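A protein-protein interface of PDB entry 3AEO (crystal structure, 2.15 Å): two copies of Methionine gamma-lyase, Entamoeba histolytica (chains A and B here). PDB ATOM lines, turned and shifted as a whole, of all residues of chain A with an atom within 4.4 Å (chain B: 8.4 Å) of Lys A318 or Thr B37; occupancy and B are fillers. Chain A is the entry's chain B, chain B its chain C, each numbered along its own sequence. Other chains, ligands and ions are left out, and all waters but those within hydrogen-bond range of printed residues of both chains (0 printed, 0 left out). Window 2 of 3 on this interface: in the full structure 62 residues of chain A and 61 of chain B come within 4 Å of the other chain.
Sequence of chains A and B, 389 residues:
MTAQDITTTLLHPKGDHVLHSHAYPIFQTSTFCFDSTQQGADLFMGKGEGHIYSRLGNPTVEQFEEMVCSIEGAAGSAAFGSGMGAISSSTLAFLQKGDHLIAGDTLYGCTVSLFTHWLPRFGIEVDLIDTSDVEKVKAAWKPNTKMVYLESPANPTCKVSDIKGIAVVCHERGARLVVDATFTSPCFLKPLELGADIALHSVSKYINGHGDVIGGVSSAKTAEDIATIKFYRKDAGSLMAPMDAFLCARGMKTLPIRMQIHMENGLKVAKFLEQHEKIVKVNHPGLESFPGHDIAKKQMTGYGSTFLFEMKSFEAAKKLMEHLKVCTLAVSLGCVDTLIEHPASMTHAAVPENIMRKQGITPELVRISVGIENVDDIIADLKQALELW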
ATOM      1  N   PHE A 314       6.600  19.010 -21.967  1.00  0.00           N
ATOM      2  CA  PHE A 314       6.734  20.366 -22.518  1.00  0.00           C
ATOM      3  C   PHE A 314       7.829  20.412 -23.578  1.00  0.00           C
ATOM      4  O   PHE A 314       7.674  21.082 -24.597  1.00  0.00           O
ATOM      5  CB  PHE A 314       7.011  21.393 -21.406  1.00  0.00           C
ATOM      6  CG  PHE A 314       7.322  22.797 -21.910  1.00  0.00           C
ATOM      7  CD1 PHE A 314       8.644  23.246 -21.997  1.00  0.00           C
ATOM      8  CD2 PHE A 314       6.301  23.670 -22.268  1.00  0.00           C
ATOM      9  CE1 PHE A 314       8.945  24.531 -22.448  1.00  0.00           C
ATOM     10  CE2 PHE A 314       6.592  24.966 -22.723  1.00  0.00           C
ATOM     11  CZ  PHE A 314       7.920  25.393 -22.808  1.00  0.00           C
ATOM     12  N   GLU A 315       8.926  19.697 -23.332  1.00  0.00           N
ATOM     13  CA  GLU A 315      10.040  19.611 -24.275  1.00  0.00           C
ATOM     14  C   GLU A 315       9.603  19.028 -25.621  1.00  0.00           C
ATOM     15  O   GLU A 315       9.974  19.557 -26.680  1.00  0.00           O
ATOM     16  CB  GLU A 315      11.197  18.797 -23.680  1.00  0.00           C
ATOM     17  CG  GLU A 315      12.582  19.330 -24.062  1.00  0.00           C
ATOM     18  CD  GLU A 315      12.856  20.742 -23.514  1.00  0.00           C
ATOM     19  OE1 GLU A 315      12.954  21.700 -24.316  1.00  0.00           O
ATOM     20  OE2 GLU A 315      12.968  20.884 -22.270  1.00  0.00           O
ATOM     21  N   ALA A 316       8.807  17.954 -25.563  1.00  0.00           N
ATOM     22  CA  ALA A 316       8.236  17.305 -26.752  1.00  0.00           C
ATOM     23  C   ALA A 316       7.235  18.201 -27.513  1.00  0.00           C
ATOM     24  O   ALA A 316       7.241  18.249 -28.746  1.00  0.00           O
ATOM     25  CB  ALA A 316       7.595  15.967 -26.377  1.00  0.00           C
ATOM     26  N   ALA A 317       6.381  18.897 -26.766  1.00  0.00           N
ATOM     27  CA  ALA A 317       5.469  19.887 -27.332  1.00  0.00           C
ATOM     28  C   ALA A 317       6.237  21.001 -28.044  1.00  0.00           C
ATOM     29  O   ALA A 317       5.871  21.390 -29.147  1.00  0.00           O
ATOM     30  CB  ALA A 317       4.553  20.465 -26.252  1.00  0.00           C
ATOM     31  N   LYS A 318       7.298  21.494 -27.402  1.00  0.00           N
ATOM     32  CA  LYS A 318       8.180  22.520 -27.955  1.00  0.00           C
ATOM     33  C   LYS A 318       8.837  22.027 -29.248  1.00  0.00           C
ATOM     34  O   LYS A 318       8.927  22.783 -30.234  1.00  0.00           O
ATOM     35  CB  LYS A 318       9.245  22.927 -26.918  1.00  0.00           C
ATOM     36  CG  LYS A 318      10.191  24.073 -27.332  1.00  0.00           C
ATOM     37  CD  LYS A 318      11.562  23.938 -26.639  1.00  0.00           C
ATOM     38  CE  LYS A 318      12.672  24.674 -27.408  1.00  0.00           C
ATOM     39  NZ  LYS A 318      12.978  26.027 -26.881  1.00  0.00           N
ATOM     40  N   LYS A 319       9.268  20.764 -29.248  1.00  0.00           N
ATOM     41  CA  LYS A 319       9.966  20.177 -30.395  1.00  0.00           C
ATOM     42  C   LYS A 319       9.043  20.032 -31.600  1.00  0.00           C
ATOM     43  O   LYS A 319       9.444  20.317 -32.733  1.00  0.00           O
ATOM     44  CB  LYS A 319      10.601  18.832 -30.032  1.00  0.00           C
ATOM     45  CG  LYS A 319      11.820  18.482 -30.868  1.00  0.00           C
ATOM     46  CD  LYS A 319      12.867  17.790 -30.012  1.00  0.00           C
ATOM     47  CE  LYS A 319      13.948  17.100 -30.843  1.00  0.00           C
ATOM     48  NZ  LYS A 319      14.574  15.956 -30.088  1.00  0.00           N
ATOM     49  N   LEU A 320       7.807  19.603 -31.343  1.00  0.00           N
ATOM     50  CA  LEU A 320       6.785  19.490 -32.386  1.00  0.00           C
ATOM     51  C   LEU A 320       6.577  20.823 -33.076  1.00  0.00           C
ATOM     52  O   LEU A 320       6.835  20.948 -34.268  1.00  0.00           O
ATOM     53  CB  LEU A 320       5.446  19.027 -31.795  1.00  0.00           C
ATOM     54  CG  LEU A 320       4.446  18.228 -32.648  1.00  0.00           C
ATOM     55  CD1 LEU A 320       3.020  18.553 -32.225  1.00  0.00           C
ATOM     56  CD2 LEU A 320       4.612  18.441 -34.147  1.00  0.00           C
ATOM     57  N   MET A 321       6.136  21.807 -32.291  1.00  0.00           N
ATOM     58  CA  MET A 321       5.700  23.127 -32.769  1.00  0.00           C
ATOM     59  C   MET A 321       6.772  23.936 -33.479  1.00  0.00           C
ATOM     60  O   MET A 321       6.454  24.835 -34.270  1.00  0.00           O
ATOM     61  CB  MET A 321       5.168  23.963 -31.605  1.00  0.00           C
ATOM     62  CG  MET A 321       3.781  23.586 -31.109  1.00  0.00           C
ATOM     63  SD  MET A 321       3.233  24.598 -29.706  1.00  0.00           S
ATOM     64  CE  MET A 321       4.529  24.299 -28.501  1.00  0.00           C
ATOM     65  N   GLU A 322       8.033  23.638 -33.184  1.00  0.00           N
ATOM     66  CA  GLU A 322       9.149  24.406 -33.726  1.00  0.00           C
ATOM     67  C   GLU A 322       9.828  23.737 -34.932  1.00  0.00           C
ATOM     68  O   GLU A 322      10.669  24.354 -35.587  1.00  0.00           O
ATOM     69  CB  GLU A 322      10.170  24.727 -32.617  1.00  0.00           C
ATOM     70  CG  GLU A 322       9.683  25.763 -31.592  1.00  0.00           C
ATOM     71  CD  GLU A 322      10.655  25.990 -30.442  1.00  0.00           C
ATOM     72  OE1 GLU A 322      11.820  25.548 -30.537  1.00  0.00           O
ATOM     73  OE2 GLU A 322      10.256  26.619 -29.435  1.00  0.00           O
ATOM     74  N   LEU A 329       3.369  28.558 -36.623  1.00  0.00           N
ATOM     75  CA  LEU A 329       3.278  28.935 -35.214  1.00  0.00           C
ATOM     76  C   LEU A 329       2.647  30.330 -35.125  1.00  0.00           C
ATOM     77  O   LEU A 329       3.260  31.317 -35.537  1.00  0.00           O
ATOM     78  CB  LEU A 329       4.663  28.934 -34.554  1.00  0.00           C
ATOM     79  CG  LEU A 329       4.860  28.104 -33.279  1.00  0.00           C
ATOM     80  CD1 LEU A 329       6.145  28.511 -32.545  1.00  0.00           C
ATOM     81  CD2 LEU A 329       3.655  28.158 -32.322  1.00  0.00           C
ATOM     82  N   MET A 346       0.359  31.233 -24.221  1.00  0.00           N
ATOM     83  CA  MET A 346      -0.106  32.149 -25.257  1.00  0.00           C
ATOM     84  C   MET A 346      -1.572  32.598 -25.053  1.00  0.00           C
ATOM     85  O   MET A 346      -1.822  33.436 -24.184  1.00  0.00           O
ATOM     86  CB  MET A 346       0.159  31.564 -26.653  1.00  0.00           C
ATOM     87  CG  MET A 346       1.618  31.179 -26.899  1.00  0.00           C
ATOM     88  SD  MET A 346       1.933  30.441 -28.518  1.00  0.00           S
ATOM     89  CE  MET A 346       3.666  29.979 -28.325  1.00  0.00           C
ATOM     90  N   PHE B  34       5.129  33.405 -35.199  1.00  0.00           N
ATOM     91  CA  PHE B  34       6.179  33.421 -34.202  1.00  0.00           C
ATOM     92  C   PHE B  34       7.373  32.669 -34.740  1.00  0.00           C
ATOM     93  O   PHE B  34       7.208  31.679 -35.464  1.00  0.00           O
ATOM     94  CB  PHE B  34       5.723  32.779 -32.895  1.00  0.00           C
ATOM     95  CG  PHE B  34       4.615  33.527 -32.192  1.00  0.00           C
ATOM     96  CD1 PHE B  34       4.573  34.931 -32.199  1.00  0.00           C
ATOM     97  CD2 PHE B  34       3.632  32.821 -31.472  1.00  0.00           C
ATOM     98  CE1 PHE B  34       3.553  35.623 -31.543  1.00  0.00           C
ATOM     99  CE2 PHE B  34       2.607  33.508 -30.798  1.00  0.00           C
ATOM    100  CZ  PHE B  34       2.569  34.922 -30.837  1.00  0.00           C
ATOM    101  N   ASP B  35       8.572  33.138 -34.379  1.00  0.00           N
ATOM    102  CA  ASP B  35       9.815  32.435 -34.692  1.00  0.00           C
ATOM    103  C   ASP B  35       9.987  31.130 -33.889  1.00  0.00           C
ATOM    104  O   ASP B  35      10.493  30.142 -34.427  1.00  0.00           O
ATOM    105  CB  ASP B  35      11.022  33.358 -34.485  1.00  0.00           C
ATOM    106  CG  ASP B  35      11.107  34.466 -35.527  1.00  0.00           C
ATOM    107  OD1 ASP B  35      10.416  34.414 -36.571  1.00  0.00           O
ATOM    108  OD2 ASP B  35      11.888  35.411 -35.301  1.00  0.00           O
ATOM    109  N   SER B  36       9.568  31.148 -32.617  1.00  0.00           N
ATOM    110  CA  SER B  36       9.719  30.018 -31.673  1.00  0.00           C
ATOM    111  C   SER B  36       8.652  30.048 -30.581  1.00  0.00           C
ATOM    112  O   SER B  36       7.934  31.035 -30.450  1.00  0.00           O
ATOM    113  CB  SER B  36      11.099  30.048 -31.007  1.00  0.00           C
ATOM    114  OG  SER B  36      11.219  31.166 -30.140  1.00  0.00           O
ATOM    115  N   THR B  37       8.555  28.970 -29.793  1.00  0.00           N
ATOM    116  CA  THR B  37       7.648  28.937 -28.644  1.00  0.00           C
ATOM    117  C   THR B  37       8.008  30.049 -27.649  1.00  0.00           C
ATOM    118  O   THR B  37       7.119  30.788 -27.202  1.00  0.00           O
ATOM    119  CB  THR B  37       7.650  27.561 -27.912  1.00  0.00           C
ATOM    120  OG1 THR B  37       7.413  26.504 -28.852  1.00  0.00           O
ATOM    121  CG2 THR B  37       6.577  27.529 -26.842  1.00  0.00           C
ATOM    122  N   GLN B  38       9.305  30.167 -27.331  1.00  0.00           N
ATOM    123  CA  GLN B  38       9.836  31.190 -26.414  1.00  0.00           C
ATOM    124  C   GLN B  38       9.521  32.625 -26.880  1.00  0.00           C
ATOM    125  O   GLN B  38       9.019  33.439 -26.106  1.00  0.00           O
ATOM    126  CB  GLN B  38      11.351  31.032 -26.244  1.00  0.00           C
ATOM    127  CG  GLN B  38      11.930  31.670 -24.972  1.00  0.00           C
ATOM    128  CD  GLN B  38      11.785  30.781 -23.728  1.00  0.00           C
ATOM    129  OE1 GLN B  38      12.782  30.291 -23.165  1.00  0.00           O
ATOM    130  NE2 GLN B  38      10.537  30.558 -23.300  1.00  0.00           N
ATOM    131  N   GLN B  39       9.824  32.926 -28.139  1.00  0.00           N
ATOM    132  CA  GLN B  39       9.624  34.276 -28.662  1.00  0.00           C
ATOM    133  C   GLN B  39       8.149  34.681 -28.543  1.00  0.00           C
ATOM    134  O   GLN B  39       7.852  35.761 -28.038  1.00  0.00           O
ATOM    135  CB  GLN B  39      10.151  34.406 -30.102  1.00  0.00           C
ATOM    136  CG  GLN B  39      10.159  35.848 -30.660  1.00  0.00           C
ATOM    137  CD  GLN B  39       9.079  36.090 -31.713  1.00  0.00           C
ATOM    138  OE1 GLN B  39       8.961  37.199 -32.276  1.00  0.00           O
ATOM    139  NE2 GLN B  39       8.279  35.057 -31.989  1.00  0.00           N
ATOM    140  N   GLY B  40       7.243  33.799 -28.979  1.00  0.00           N
ATOM    141  CA  GLY B  40       5.796  33.972 -28.797  1.00  0.00           C
ATOM    142  C   GLY B  40       5.352  34.118 -27.343  1.00  0.00           C
ATOM    143  O   GLY B  40       4.635  35.078 -27.009  1.00  0.00           O
ATOM    144  N   ALA B  41       5.772  33.174 -26.488  1.00  0.00           N
ATOM    145  CA  ALA B  41       5.532  33.254 -25.037  1.00  0.00           C
ATOM    146  C   ALA B  41       6.009  34.586 -24.449  1.00  0.00           C
ATOM    147  O   ALA B  41       5.297  35.207 -23.659  1.00  0.00           O
ATOM    148  CB  ALA B  41       6.195  32.063 -24.280  1.00  0.00           C
ATOM    149  N   ASP B  42       7.209  35.012 -24.838  1.00  0.00           N
ATOM    150  CA  ASP B  42       7.785  36.271 -24.368  1.00  0.00           C
ATOM    151  C   ASP B  42       6.937  37.508 -24.716  1.00  0.00           C
ATOM    152  O   ASP B  42       6.780  38.409 -23.881  1.00  0.00           O
ATOM    153  CB  ASP B  42       9.226  36.437 -24.886  1.00  0.00           C
ATOM    154  CG  ASP B  42      10.241  35.621 -24.077  1.00  0.00           C
ATOM    155  OD1 ASP B  42       9.935  35.216 -22.936  1.00  0.00           O
ATOM    156  OD2 ASP B  42      11.355  35.382 -24.583  1.00  0.00           O
ATOM    157  N   LEU B  43       6.390  37.540 -25.937  1.00  0.00           N
ATOM    158  CA  LEU B  43       5.605  38.690 -26.407  1.00  0.00           C
ATOM    159  C   LEU B  43       4.320  38.837 -25.605  1.00  0.00           C
ATOM    160  O   LEU B  43       3.860  39.947 -25.352  1.00  0.00           O
ATOM    161  CB  LEU B  43       5.294  38.569 -27.897  1.00  0.00           C
ATOM    162  CG  LEU B  43       6.409  38.960 -28.868  1.00  0.00           C
ATOM    163  CD1 LEU B  43       5.983  38.650 -30.312  1.00  0.00           C
ATOM    164  CD2 LEU B  43       6.752  40.454 -28.714  1.00  0.00           C
ATOM    165  N   PHE B  44       3.757  37.707 -25.180  1.00  0.00           N
ATOM    166  CA  PHE B  44       2.618  37.710 -24.258  1.00  0.00           C
ATOM    167  C   PHE B  44       2.943  38.220 -22.840  1.00  0.00           C
ATOM    168  O   PHE B  44       2.030  38.498 -22.076  1.00  0.00           O
ATOM    169  CB  PHE B  44       1.960  36.314 -24.198  1.00  0.00           C
ATOM    170  CG  PHE B  44       0.869  36.111 -25.231  1.00  0.00           C
ATOM    171  CD1 PHE B  44       1.127  35.412 -26.405  1.00  0.00           C
ATOM    172  CD2 PHE B  44      -0.413  36.632 -25.022  1.00  0.00           C
ATOM    173  CE1 PHE B  44       0.130  35.231 -27.354  1.00  0.00           C
ATOM    174  CE2 PHE B  44      -1.419  36.461 -25.961  1.00  0.00           C
ATOM    175  CZ  PHE B  44      -1.150  35.755 -27.133  1.00  0.00           C
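NZ of Lys A318 lies within salt-bridge range of OE2 of Glu A322.
The side-chain hydroxyl (OG) of Ser B36 is in hydrogen-bond range of the backbone NH (N) of Gln B39, 3.0 Å away.
No position is printed for both chains.
OE2 of Glu A322 lies within hydrogen-bond range of OG1 of Thr B37, 2.9 Å away.
The backbone NH (N) of Phe B34 is in hydrogen-bond range of the backbone carbonyl oxygen (O) of Leu A329, 2.8 Å away.
Of the 11 printed residues of chain B, 4 touch a printed residue of chain A.
Hydrophobic or aromatic side chains of chain A that line the printed part of chain B: Met A321, Leu A329 and Met A346.
Among the printed residues, pairs that only touch across the chains: Lys A318 with Thr B37, Met A321 with Thr B37, Glu A322 with Ser B36, Leu A329 with Ser B36, Leu A329 with Thr B37, Met A346 with Phe B34, Met A346 with Thr B37 and Met A346 with Phe B44.
Printed residues of chain B within 4 Å of Lys A318: Thr B37.
Printed residues of chain A within 4 Å of Thr B37: Lys A318, Met A321, Glu A322, Leu A329 and Met A346.
Ala A317 touches none of the printed residues of chain B.
Of the printed residues of chain B, Met A321 touches Thr B37 (3.6 Å).
Of the printed residues of chain A, Ser B36 touches Glu A322 and Leu A329.
Printed residues of chain B within 4 Å of Glu A322: Ser B36 (3.9 Å) and Thr B37 (2.9 Å).
Of the printed residues of chain B, Met A346 touches Phe B34 (3.9 Å), Thr B37 (3.7 Å) and Phe B44 (3.5 Å).
Leu A320 touches none of the printed residues of chain B.
The nearest printed residue of chain B that does not touch Lys A318 is Gln B38 (5.3 Å).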
